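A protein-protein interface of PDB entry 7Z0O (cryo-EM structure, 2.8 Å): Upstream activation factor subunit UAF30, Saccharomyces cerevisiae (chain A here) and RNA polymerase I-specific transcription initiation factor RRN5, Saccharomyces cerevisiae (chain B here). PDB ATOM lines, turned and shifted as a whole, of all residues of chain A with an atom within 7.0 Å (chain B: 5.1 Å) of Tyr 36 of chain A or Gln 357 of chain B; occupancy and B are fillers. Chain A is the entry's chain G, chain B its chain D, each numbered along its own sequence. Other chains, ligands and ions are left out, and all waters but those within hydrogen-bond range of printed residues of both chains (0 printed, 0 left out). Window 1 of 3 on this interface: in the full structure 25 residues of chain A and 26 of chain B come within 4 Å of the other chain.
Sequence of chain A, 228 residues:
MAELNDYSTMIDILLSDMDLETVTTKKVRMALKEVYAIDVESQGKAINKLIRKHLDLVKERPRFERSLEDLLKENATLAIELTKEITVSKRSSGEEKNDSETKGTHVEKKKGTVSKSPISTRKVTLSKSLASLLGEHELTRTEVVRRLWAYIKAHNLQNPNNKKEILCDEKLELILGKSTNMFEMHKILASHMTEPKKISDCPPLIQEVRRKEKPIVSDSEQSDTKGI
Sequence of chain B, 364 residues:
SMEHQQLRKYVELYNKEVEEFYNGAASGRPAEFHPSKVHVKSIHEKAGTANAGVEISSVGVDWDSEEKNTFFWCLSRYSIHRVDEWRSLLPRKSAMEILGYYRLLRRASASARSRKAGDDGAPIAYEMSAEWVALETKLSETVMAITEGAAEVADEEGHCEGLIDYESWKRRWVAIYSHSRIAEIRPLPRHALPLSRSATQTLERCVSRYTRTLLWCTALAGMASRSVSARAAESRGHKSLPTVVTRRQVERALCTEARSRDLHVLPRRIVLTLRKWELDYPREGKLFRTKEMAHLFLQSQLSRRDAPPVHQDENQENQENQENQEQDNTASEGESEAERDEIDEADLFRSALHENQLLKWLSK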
ATOM      1  N   THR A   9      10.775  31.407   4.120  1.00  0.00           N
ATOM      2  CA  THR A   9      10.101  32.020   2.981  1.00  0.00           C
ATOM      3  C   THR A   9       8.946  31.156   2.494  1.00  0.00           C
ATOM      4  O   THR A   9       7.893  31.673   2.104  1.00  0.00           O
ATOM      5  CB  THR A   9      11.097  32.264   1.848  1.00  0.00           C
ATOM      6  OG1 THR A   9      12.314  32.795   2.386  1.00  0.00           O
ATOM      7  CG2 THR A   9      10.523  33.247   0.841  1.00  0.00           C
ATOM      8  N   MET A  10       9.129  29.834   2.502  1.00  0.00           N
ATOM      9  CA  MET A  10       8.059  28.935   2.087  1.00  0.00           C
ATOM     10  C   MET A  10       6.852  29.054   3.007  1.00  0.00           C
ATOM     11  O   MET A  10       5.706  29.076   2.542  1.00  0.00           O
ATOM     12  CB  MET A  10       8.571  27.496   2.061  1.00  0.00           C
ATOM     13  CG  MET A  10       9.456  27.172   0.875  1.00  0.00           C
ATOM     14  SD  MET A  10      10.229  25.553   1.028  1.00  0.00           S
ATOM     15  CE  MET A  10      10.812  25.300  -0.644  1.00  0.00           C
ATOM     16  N   ILE A  11       7.089  29.132   4.318  1.00  0.00           N
ATOM     17  CA  ILE A  11       5.989  29.254   5.271  1.00  0.00           C
ATOM     18  C   ILE A  11       5.261  30.577   5.078  1.00  0.00           C
ATOM     19  O   ILE A  11       4.027  30.638   5.136  1.00  0.00           O
ATOM     20  CB  ILE A  11       6.512  29.099   6.710  1.00  0.00           C
ATOM     21  CG1 ILE A  11       7.126  27.714   6.902  1.00  0.00           C
ATOM     22  CG2 ILE A  11       5.393  29.320   7.712  1.00  0.00           C
ATOM     23  CD1 ILE A  11       8.162  27.656   7.993  1.00  0.00           C
ATOM     24  N   ILE A  13       4.941  32.335   2.328  1.00  0.00           N
ATOM     25  CA  ILE A  13       4.132  32.276   1.114  1.00  0.00           C
ATOM     26  C   ILE A  13       2.860  31.475   1.357  1.00  0.00           C
ATOM     27  O   ILE A  13       1.768  31.871   0.930  1.00  0.00           O
ATOM     28  CB  ILE A  13       4.957  31.691  -0.047  1.00  0.00           C
ATOM     29  CG1 ILE A  13       6.066  32.660  -0.451  1.00  0.00           C
ATOM     30  CG2 ILE A  13       4.066  31.389  -1.236  1.00  0.00           C
ATOM     31  CD1 ILE A  13       7.072  32.066  -1.402  1.00  0.00           C
ATOM     32  N   LEU A  14       2.978  30.337   2.046  1.00  0.00           N
ATOM     33  CA  LEU A  14       1.816  29.486   2.274  1.00  0.00           C
ATOM     34  C   LEU A  14       0.772  30.182   3.136  1.00  0.00           C
ATOM     35  O   LEU A  14      -0.430  30.090   2.863  1.00  0.00           O
ATOM     36  CB  LEU A  14       2.250  28.174   2.924  1.00  0.00           C
ATOM     37  CG  LEU A  14       2.946  27.158   2.018  1.00  0.00           C
ATOM     38  CD1 LEU A  14       3.274  25.897   2.794  1.00  0.00           C
ATOM     39  CD2 LEU A  14       2.086  26.839   0.813  1.00  0.00           C
ATOM     40  N   LEU A  15       1.210  30.884   4.183  1.00  0.00           N
ATOM     41  CA  LEU A  15       0.273  31.511   5.107  1.00  0.00           C
ATOM     42  C   LEU A  15      -0.469  32.685   4.487  1.00  0.00           C
ATOM     43  O   LEU A  15      -1.535  33.060   4.985  1.00  0.00           O
ATOM     44  CB  LEU A  15       1.009  31.975   6.364  1.00  0.00           C
ATOM     45  CG  LEU A  15       1.477  30.866   7.303  1.00  0.00           C
ATOM     46  CD1 LEU A  15       2.160  31.455   8.524  1.00  0.00           C
ATOM     47  CD2 LEU A  15       0.307  29.988   7.709  1.00  0.00           C
ATOM     48  N   SER A  16       0.064  33.272   3.415  1.00  0.00           N
ATOM     49  CA  SER A  16      -0.536  34.465   2.832  1.00  0.00           C
ATOM     50  C   SER A  16      -1.823  34.179   2.069  1.00  0.00           C
ATOM     51  O   SER A  16      -2.512  35.130   1.685  1.00  0.00           O
ATOM     52  CB  SER A  16       0.465  35.151   1.904  1.00  0.00           C
ATOM     53  OG  SER A  16      -0.111  36.283   1.279  1.00  0.00           O
ATOM     54  N   ASP A  17      -2.168  32.913   1.839  1.00  0.00           N
ATOM     55  CA  ASP A  17      -3.313  32.572   1.004  1.00  0.00           C
ATOM     56  C   ASP A  17      -4.265  31.577   1.656  1.00  0.00           C
ATOM     57  O   ASP A  17      -5.123  31.018   0.963  1.00  0.00           O
ATOM     58  CB  ASP A  17      -2.836  32.027  -0.344  1.00  0.00           C
ATOM     59  CG  ASP A  17      -2.521  33.126  -1.336  1.00  0.00           C
ATOM     60  OD1 ASP A  17      -3.433  33.913  -1.665  1.00  0.00           O
ATOM     61  OD2 ASP A  17      -1.360  33.206  -1.790  1.00  0.00           O
ATOM     62  N   MET A  18      -4.143  31.338   2.958  1.00  0.00           N
ATOM     63  CA  MET A  18      -5.062  30.466   3.673  1.00  0.00           C
ATOM     64  C   MET A  18      -5.670  31.225   4.842  1.00  0.00           C
ATOM     65  O   MET A  18      -4.981  31.989   5.524  1.00  0.00           O
ATOM     66  CB  MET A  18      -4.362  29.194   4.175  1.00  0.00           C
ATOM     67  CG  MET A  18      -3.122  29.441   5.013  1.00  0.00           C
ATOM     68  SD  MET A  18      -2.565  27.956   5.870  1.00  0.00           S
ATOM     69  CE  MET A  18      -1.785  27.059   4.531  1.00  0.00           C
ATOM     70  N   ALA A  31       0.958  21.292   4.035  1.00  0.00           N
ATOM     71  CA  ALA A  31       0.978  22.108   2.825  1.00  0.00           C
ATOM     72  C   ALA A  31       2.397  22.292   2.302  1.00  0.00           C
ATOM     73  O   ALA A  31       2.599  22.488   1.098  1.00  0.00           O
ATOM     74  CB  ALA A  31       0.326  23.463   3.094  1.00  0.00           C
ATOM     75  N   LEU A  32       3.389  22.250   3.191  1.00  0.00           N
ATOM     76  CA  LEU A  32       4.777  22.369   2.755  1.00  0.00           C
ATOM     77  C   LEU A  32       5.168  21.202   1.859  1.00  0.00           C
ATOM     78  O   LEU A  32       5.844  21.384   0.841  1.00  0.00           O
ATOM     79  CB  LEU A  32       5.705  22.451   3.966  1.00  0.00           C
ATOM     80  CG  LEU A  32       5.956  23.842   4.545  1.00  0.00           C
ATOM     81  CD1 LEU A  32       6.732  23.737   5.844  1.00  0.00           C
ATOM     82  CD2 LEU A  32       6.697  24.710   3.548  1.00  0.00           C
ATOM     83  N   LYS A  33       4.755  19.989   2.229  1.00  0.00           N
ATOM     84  CA  LYS A  33       5.061  18.824   1.409  1.00  0.00           C
ATOM     85  C   LYS A  33       4.221  18.796   0.141  1.00  0.00           C
ATOM     86  O   LYS A  33       4.672  18.291  -0.892  1.00  0.00           O
ATOM     87  CB  LYS A  33       4.845  17.546   2.218  1.00  0.00           C
ATOM     88  CG  LYS A  33       5.217  16.273   1.482  1.00  0.00           C
ATOM     89  CD  LYS A  33       5.066  15.055   2.372  1.00  0.00           C
ATOM     90  CE  LYS A  33       5.281  13.774   1.587  1.00  0.00           C
ATOM     91  NZ  LYS A  33       6.672  13.676   1.066  1.00  0.00           N
ATOM     92  N   GLU A  34       3.003  19.333   0.193  1.00  0.00           N
ATOM     93  CA  GLU A  34       2.121  19.288  -0.966  1.00  0.00           C
ATOM     94  C   GLU A  34       2.569  20.233  -2.074  1.00  0.00           C
ATOM     95  O   GLU A  34       2.395  19.917  -3.255  1.00  0.00           O
ATOM     96  CB  GLU A  34       0.687  19.613  -0.547  1.00  0.00           C
ATOM     97  CG  GLU A  34      -0.309  19.652  -1.694  1.00  0.00           C
ATOM     98  CD  GLU A  34      -0.869  18.285  -2.035  1.00  0.00           C
ATOM     99  OE1 GLU A  34      -0.278  17.271  -1.609  1.00  0.00           O
ATOM    100  OE2 GLU A  34      -1.904  18.223  -2.731  1.00  0.00           O
ATOM    101  N   VAL A  35       3.142  21.381  -1.728  1.00  0.00           N
ATOM    102  CA  VAL A  35       3.518  22.380  -2.717  1.00  0.00           C
ATOM    103  C   VAL A  35       4.999  22.307  -3.061  1.00  0.00           C
ATOM    104  O   VAL A  35       5.368  22.382  -4.233  1.00  0.00           O
ATOM    105  CB  VAL A  35       3.131  23.791  -2.225  1.00  0.00           C
ATOM    106  CG1 VAL A  35       3.381  24.815  -3.315  1.00  0.00           C
ATOM    107  CG2 VAL A  35       1.680  23.816  -1.793  1.00  0.00           C
ATOM    108  N   TYR A  36       5.862  22.159  -2.058  1.00  0.00           N
ATOM    109  CA  TYR A  36       7.302  22.209  -2.265  1.00  0.00           C
ATOM    110  C   TYR A  36       7.992  20.868  -2.070  1.00  0.00           C
ATOM    111  O   TYR A  36       9.207  20.782  -2.271  1.00  0.00           O
ATOM    112  CB  TYR A  36       7.926  23.249  -1.332  1.00  0.00           C
ATOM    113  CG  TYR A  36       7.287  24.608  -1.450  1.00  0.00           C
ATOM    114  CD1 TYR A  36       7.399  25.345  -2.617  1.00  0.00           C
ATOM    115  CD2 TYR A  36       6.565  25.151  -0.400  1.00  0.00           C
ATOM    116  CE1 TYR A  36       6.814  26.584  -2.735  1.00  0.00           C
ATOM    117  CE2 TYR A  36       5.977  26.393  -0.509  1.00  0.00           C
ATOM    118  CZ  TYR A  36       6.106  27.105  -1.678  1.00  0.00           C
ATOM    119  OH  TYR A  36       5.524  28.343  -1.797  1.00  0.00           O
ATOM    120  N   ALA A  37       7.255  19.829  -1.677  1.00  0.00           N
ATOM    121  CA  ALA A  37       7.786  18.471  -1.555  1.00  0.00           C
ATOM    122  C   ALA A  37       8.977  18.399  -0.605  1.00  0.00           C
ATOM    123  O   ALA A  37       9.825  17.512  -0.725  1.00  0.00           O
ATOM    124  CB  ALA A  37       8.163  17.897  -2.923  1.00  0.00           C
ATOM    125  N   ILE A  38       9.058  19.320   0.346  1.00  0.00           N
ATOM    126  CA  ILE A  38      10.133  19.293   1.328  1.00  0.00           C
ATOM    127  C   ILE A  38       9.810  18.246   2.384  1.00  0.00           C
ATOM    128  O   ILE A  38       8.653  18.076   2.783  1.00  0.00           O
ATOM    129  CB  ILE A  38      10.359  20.699   1.926  1.00  0.00           C
ATOM    130  CG1 ILE A  38       9.230  21.140   2.867  1.00  0.00           C
ATOM    131  CG2 ILE A  38      10.542  21.723   0.819  1.00  0.00           C
ATOM    132  CD1 ILE A  38       9.420  20.764   4.326  1.00  0.00           C
ATOM    133  N   ASP A  39      10.834  17.514   2.818  1.00  0.00           N
ATOM    134  CA  ASP A  39      10.629  16.437   3.777  1.00  0.00           C
ATOM    135  C   ASP A  39      10.461  16.998   5.182  1.00  0.00           C
ATOM    136  O   ASP A  39      11.387  17.600   5.735  1.00  0.00           O
ATOM    137  CB  ASP A  39      11.792  15.446   3.730  1.00  0.00           C
ATOM    138  CG  ASP A  39      11.949  14.674   5.021  1.00  0.00           C
ATOM    139  OD1 ASP A  39      11.167  13.728   5.249  1.00  0.00           O
ATOM    140  OD2 ASP A  39      12.853  15.017   5.809  1.00  0.00           O
ATOM    141  N   ARG A  66      -8.572  36.744  -2.716  1.00  0.00           N
ATOM    142  CA  ARG A  66      -8.533  37.057  -4.135  1.00  0.00           C
ATOM    143  C   ARG A  66      -9.202  35.939  -4.918  1.00  0.00           C
ATOM    144  O   ARG A  66      -8.981  34.756  -4.640  1.00  0.00           O
ATOM    145  CB  ARG A  66      -7.097  37.267  -4.626  1.00  0.00           C
ATOM    146  CG  ARG A  66      -6.102  36.241  -4.121  1.00  0.00           C
ATOM    147  CD  ARG A  66      -4.693  36.606  -4.554  1.00  0.00           C
ATOM    148  NE  ARG A  66      -3.692  35.718  -3.977  1.00  0.00           N
ATOM    149  CZ  ARG A  66      -2.399  35.763  -4.270  1.00  0.00           C
ATOM    150  NH1 ARG A  66      -1.917  36.641  -5.133  1.00  0.00           N
ATOM    151  NH2 ARG A  66      -1.571  34.904  -3.683  1.00  0.00           N
ATOM    152  N   LEU A  71      -5.966  35.517  -9.386  1.00  0.00           N
ATOM    153  CA  LEU A  71      -4.885  34.536  -9.396  1.00  0.00           C
ATOM    154  C   LEU A  71      -4.390  34.274 -10.813  1.00  0.00           C
ATOM    155  O   LEU A  71      -3.180  34.169 -11.044  1.00  0.00           O
ATOM    156  CB  LEU A  71      -5.352  33.235  -8.746  1.00  0.00           C
ATOM    157  CG  LEU A  71      -5.311  33.185  -7.220  1.00  0.00           C
ATOM    158  CD1 LEU A  71      -5.655  31.792  -6.722  1.00  0.00           C
ATOM    159  CD2 LEU A  71      -3.950  33.616  -6.711  1.00  0.00           C
ATOM    160  N   ASN A  75      -0.620  35.080 -11.992  1.00  0.00           N
ATOM    161  CA  ASN A  75       0.197  33.932 -12.372  1.00  0.00           C
ATOM    162  C   ASN A  75       0.822  34.135 -13.743  1.00  0.00           C
ATOM    163  O   ASN A  75       1.989  33.789 -13.960  1.00  0.00           O
ATOM    164  CB  ASN A  75      -0.639  32.652 -12.356  1.00  0.00           C
ATOM    165  CG  ASN A  75      -0.896  32.144 -10.957  1.00  0.00           C
ATOM    166  OD1 ASN A  75      -0.582  32.813  -9.976  1.00  0.00           O
ATOM    167  ND2 ASN A  75      -1.475  30.954 -10.856  1.00  0.00           N
ATOM    168  N   LEU A  78       3.775  36.576 -13.356  1.00  0.00           N
ATOM    169  CA  LEU A  78       4.961  35.959 -12.771  1.00  0.00           C
ATOM    170  C   LEU A  78       5.630  35.004 -13.750  1.00  0.00           C
ATOM    171  O   LEU A  78       6.863  34.940 -13.820  1.00  0.00           O
ATOM    172  CB  LEU A  78       4.592  35.231 -11.480  1.00  0.00           C
ATOM    173  CG  LEU A  78       4.254  36.103 -10.272  1.00  0.00           C
ATOM    174  CD1 LEU A  78       3.602  35.271  -9.184  1.00  0.00           C
ATOM    175  CD2 LEU A  78       5.501  36.790  -9.749  1.00  0.00           C
ATOM    176  N   LEU B  13      13.399  21.069  -6.185  1.00  0.00           N
ATOM    177  CA  LEU B  13      12.004  20.675  -6.346  1.00  0.00           C
ATOM    178  C   LEU B  13      11.896  19.391  -7.156  1.00  0.00           C
ATOM    179  O   LEU B  13      11.133  18.483  -6.807  1.00  0.00           O
ATOM    180  CB  LEU B  13      11.213  21.800  -7.008  1.00  0.00           C
ATOM    181  CG  LEU B  13       9.812  21.442  -7.504  1.00  0.00           C
ATOM    182  CD1 LEU B  13       8.901  21.102  -6.339  1.00  0.00           C
ATOM    183  CD2 LEU B  13       9.231  22.575  -8.327  1.00  0.00           C
ATOM    184  N   LYS B  16      13.440  16.408  -4.962  1.00  0.00           N
ATOM    185  CA  LYS B  16      12.560  15.981  -3.880  1.00  0.00           C
ATOM    186  C   LYS B  16      11.335  15.257  -4.422  1.00  0.00           C
ATOM    187  O   LYS B  16      10.852  14.296  -3.812  1.00  0.00           O
ATOM    188  CB  LYS B  16      12.148  17.183  -3.036  1.00  0.00           C
ATOM    189  CG  LYS B  16      13.284  17.777  -2.226  1.00  0.00           C
ATOM    190  CD  LYS B  16      12.864  19.066  -1.551  1.00  0.00           C
ATOM    191  CE  LYS B  16      14.056  19.776  -0.938  1.00  0.00           C
ATOM    192  NZ  LYS B  16      14.657  18.990   0.173  1.00  0.00           N
ATOM    193  N   LEU B 353      -4.104  28.397  -7.292  1.00  0.00           N
ATOM    194  CA  LEU B 353      -3.380  28.753  -6.079  1.00  0.00           C
ATOM    195  C   LEU B 353      -2.073  27.979  -5.967  1.00  0.00           C
ATOM    196  O   LEU B 353      -1.047  28.539  -5.566  1.00  0.00           O
ATOM    197  CB  LEU B 353      -4.256  28.505  -4.854  1.00  0.00           C
ATOM    198  CG  LEU B 353      -3.655  28.937  -3.519  1.00  0.00           C
ATOM    199  CD1 LEU B 353      -3.362  30.423  -3.539  1.00  0.00           C
ATOM    200  CD2 LEU B 353      -4.586  28.584  -2.375  1.00  0.00           C
ATOM    201  N   HIS B 354      -2.092  26.691  -6.315  1.00  0.00           N
ATOM    202  CA  HIS B 354      -0.879  25.882  -6.239  1.00  0.00           C
ATOM    203  C   HIS B 354       0.197  26.414  -7.175  1.00  0.00           C
ATOM    204  O   HIS B 354       1.373  26.490  -6.802  1.00  0.00           O
ATOM    205  CB  HIS B 354      -1.202  24.426  -6.564  1.00  0.00           C
ATOM    206  CG  HIS B 354      -0.012  23.521  -6.523  1.00  0.00           C
ATOM    207  ND1 HIS B 354       0.826  23.344  -7.601  1.00  0.00           N
ATOM    208  CD2 HIS B 354       0.479  22.739  -5.534  1.00  0.00           C
ATOM    209  CE1 HIS B 354       1.783  22.494  -7.279  1.00  0.00           C
ATOM    210  NE2 HIS B 354       1.595  22.112  -6.029  1.00  0.00           N
ATOM    211  N   GLU B 355      -0.186  26.785  -8.397  1.00  0.00           N
ATOM    212  CA  GLU B 355       0.768  27.392  -9.316  1.00  0.00           C
ATOM    213  C   GLU B 355       1.256  28.733  -8.790  1.00  0.00           C
ATOM    214  O   GLU B 355       2.424  29.093  -8.970  1.00  0.00           O
ATOM    215  CB  GLU B 355       0.129  27.553 -10.694  1.00  0.00           C
ATOM    216  CG  GLU B 355       1.082  28.000 -11.779  1.00  0.00           C
ATOM    217  CD  GLU B 355       0.372  28.275 -13.087  1.00  0.00           C
ATOM    218  OE1 GLU B 355      -0.620  27.578 -13.383  1.00  0.00           O
ATOM    219  OE2 GLU B 355       0.803  29.189 -13.819  1.00  0.00           O
ATOM    220  N   ASN B 356       0.369  29.489  -8.140  1.00  0.00           N
ATOM    221  CA  ASN B 356       0.744  30.795  -7.610  1.00  0.00           C
ATOM    222  C   ASN B 356       1.820  30.675  -6.540  1.00  0.00           C
ATOM    223  O   ASN B 356       2.774  31.460  -6.516  1.00  0.00           O
ATOM    224  CB  ASN B 356      -0.489  31.498  -7.051  1.00  0.00           C
ATOM    225  CG  ASN B 356      -0.266  32.973  -6.839  1.00  0.00           C
ATOM    226  OD1 ASN B 356       0.245  33.393  -5.804  1.00  0.00           O
ATOM    227  ND2 ASN B 356      -0.640  33.770  -7.825  1.00  0.00           N
ATOM    228  N   GLN B 357       1.683  29.700  -5.641  1.00  0.00           N
ATOM    229  CA  GLN B 357       2.671  29.534  -4.581  1.00  0.00           C
ATOM    230  C   GLN B 357       4.005  29.044  -5.127  1.00  0.00           C
ATOM    231  O   GLN B 357       5.054  29.327  -4.540  1.00  0.00           O
ATOM    232  CB  GLN B 357       2.135  28.575  -3.520  1.00  0.00           C
ATOM    233  CG  GLN B 357       0.785  28.988  -2.966  1.00  0.00           C
ATOM    234  CD  GLN B 357       0.199  27.967  -2.019  1.00  0.00           C
ATOM    235  OE1 GLN B 357       0.212  26.768  -2.293  1.00  0.00           O
ATOM    236  NE2 GLN B 357      -0.330  28.438  -0.897  1.00  0.00           N
ATOM    237  N   LEU B 358       3.987  28.305  -6.237  1.00  0.00           N
ATOM    238  CA  LEU B 358       5.237  27.877  -6.855  1.00  0.00           C
ATOM    239  C   LEU B 358       5.932  29.038  -7.554  1.00  0.00           C
ATOM    240  O   LEU B 358       7.156  29.185  -7.456  1.00  0.00           O
ATOM    241  CB  LEU B 358       4.977  26.741  -7.841  1.00  0.00           C
ATOM    242  CG  LEU B 358       4.964  25.327  -7.265  1.00  0.00           C
ATOM    243  CD1 LEU B 358       4.603  24.322  -8.341  1.00  0.00           C
ATOM    244  CD2 LEU B 358       6.307  24.993  -6.646  1.00  0.00           C
ATOM    245  N   LEU B 359       5.171  29.869  -8.269  1.00  0.00           N
ATOM    246  CA  LEU B 359       5.768  31.003  -8.966  1.00  0.00           C
ATOM    247  C   LEU B 359       6.357  32.010  -7.986  1.00  0.00           C
ATOM    248  O   LEU B 359       7.443  32.551  -8.224  1.00  0.00           O
ATOM    249  CB  LEU B 359       4.731  31.674  -9.864  1.00  0.00           C
ATOM    250  CG  LEU B 359       4.331  30.905 -11.121  1.00  0.00           C
ATOM    251  CD1 LEU B 359       3.134  31.558 -11.779  1.00  0.00           C
ATOM    252  CD2 LEU B 359       5.494  30.824 -12.087  1.00  0.00           C
ATOM    253  N   LYS B 360       5.654  32.280  -6.885  1.00  0.00           N
ATOM    254  CA  LYS B 360       6.180  33.199  -5.881  1.00  0.00           C
ATOM    255  C   LYS B 360       7.457  32.655  -5.259  1.00  0.00           C
ATOM    256  O   LYS B 360       8.393  33.412  -4.978  1.00  0.00           O
ATOM    257  CB  LYS B 360       5.130  33.458  -4.803  1.00  0.00           C
ATOM    258  CG  LYS B 360       4.017  34.391  -5.231  1.00  0.00           C
ATOM    259  CD  LYS B 360       3.245  34.903  -4.029  1.00  0.00           C
ATOM    260  CE  LYS B 360       2.077  35.769  -4.456  1.00  0.00           C
ATOM    261  NZ  LYS B 360       2.520  36.905  -5.307  1.00  0.00           N
ATOM    262  N   TRP B 361       7.508  31.344  -5.029  1.00  0.00           N
ATOM    263  CA  TRP B 361       8.700  30.726  -4.461  1.00  0.00           C
ATOM    264  C   TRP B 361       9.898  30.875  -5.389  1.00  0.00           C
ATOM    265  O   TRP B 361      11.017  31.133  -4.934  1.00  0.00           O
ATOM    266  CB  TRP B 361       8.414  29.257  -4.163  1.00  0.00           C
ATOM    267  CG  TRP B 361       9.606  28.366  -4.163  1.00  0.00           C
ATOM    268  CD1 TRP B 361       9.823  27.295  -4.978  1.00  0.00           C
ATOM    269  CD2 TRP B 361      10.733  28.436  -3.285  1.00  0.00           C
ATOM    270  NE1 TRP B 361      11.023  26.704  -4.674  1.00  0.00           N
ATOM    271  CE2 TRP B 361      11.601  27.385  -3.638  1.00  0.00           C
ATOM    272  CE3 TRP B 361      11.098  29.290  -2.242  1.00  0.00           C
ATOM    273  CZ2 TRP B 361      12.809  27.167  -2.986  1.00  0.00           C
ATOM    274  CZ3 TRP B 361      12.296  29.070  -1.596  1.00  0.00           C
ATOM    275  CH2 TRP B 361      13.137  28.018  -1.971  1.00  0.00           C
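The backbone carbonyl oxygen (O) of Gln 357 of chain B is in hydrogen-bond range of the side-chain hydroxyl (OH) of Tyr 36 of chain A (3.0 Å).
The side-chain amide oxygen of Asn 75 of chain A sits close to the side-chain amide nitrogen of Asn 356 of chain B, at 2.4 Å.
The side-chain amide oxygen (OD1) of Asn 356 of chain B lies within hydrogen-bond range of the guanidinium group (NH2) of Arg 66 of chain A (3.2 Å).
The backbone carbonyl oxygen (O) of Leu 32 of chain A lies within hydrogen-bond range of the backbone NH (N) of Ala 37 of chain A (3.3 Å).
O of Leu 71 of chain A lies close to OD1 of Asn 75 of chain A (3.1 Å).
OD2 of Asp 17 of chain A lies within salt-bridge range of NH2 of Arg 66 of chain A.
Trp 361 of chain B touches Met 10 of chain A (CZ2 to CE, 3.6 Å).
CD1 of Ile 13 of chain A touches C of Lys 360 of chain B (3.9 Å).
Ile 13 of chain A touches Trp 361 of chain B.
CD2 of Leu 14 of chain A touches NE2 of Gln 357 of chain B, at 3.4 Å.
Leu 353 of chain B touches Asp 17 of chain A.
Glu 34 of chain A touches His 354 of chain B.
Val 35 of chain A touches His 354 of chain B.
Lys 16 of chain B touches Ile 38 of chain A (CD to CA, 3.97 Å).
CD1 of Leu 71 of chain A touches N of Leu 353 of chain B, at 3.8 Å.
CD1 of Leu 359 of chain B touches O of Asn 75 of chain A, 3.3 Å away.
Of the printed residues of chain B, Met 10 of chain A touches Trp 361 (3.6 Å).
Met 18 of chain A touches none of the printed residues of chain B.
Leu 32 of chain A touches none of the printed residues of chain B.
Tyr 36 of chain A touches just these residues of chain B: Gln 357 (3.0 Å) and Trp 361 (3.4 Å).
Of the printed residues of chain B, Arg 66 of chain A touches Asn 356 and Lys 360.
Printed residues of chain A within 4 Å of His 354 of chain B: Glu 34 (3.6 Å) and Val 35 (3.8 Å).
Printed residues of chain A within 4 Å of Lys 360 of chain B: Ile 13 and Arg 66.
The nearest printed residue of chain B that does not touch Tyr 36 of chain A is Leu 13 of chain B (4.1 Å).
Of the 11 printed residues of chain B, 10 touch a printed residue of chain A.
Printed residues of chain B that touch a printed residue of chain A: Lys 16, Leu 353, His 354, Glu 355, Asn 356, Gln 357, Leu 358, Leu 359, Lys 360 and Trp 361.
Hydrophobic or aromatic side chains of chain B within 4 Å of the printed part of chain A: Leu 353, His 354, Leu 358, Leu 359 and Trp 361.
Of the 22 printed residues of chain A, 13 touch a printed residue of chain B.
Printed residues of chain A that touch a printed residue of chain B: Met 10, Ile 13, Leu 14, Asp 17, Glu 34, Val 35, Tyr 36, Ala 37, Ile 38, Arg 66, Leu 71, Asn 75 and Leu 78.
Among the printed residues, no Asp or Glu carboxylate lies within 4 Å of a Lys or Arg side-chain nitrogen of the other chain.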
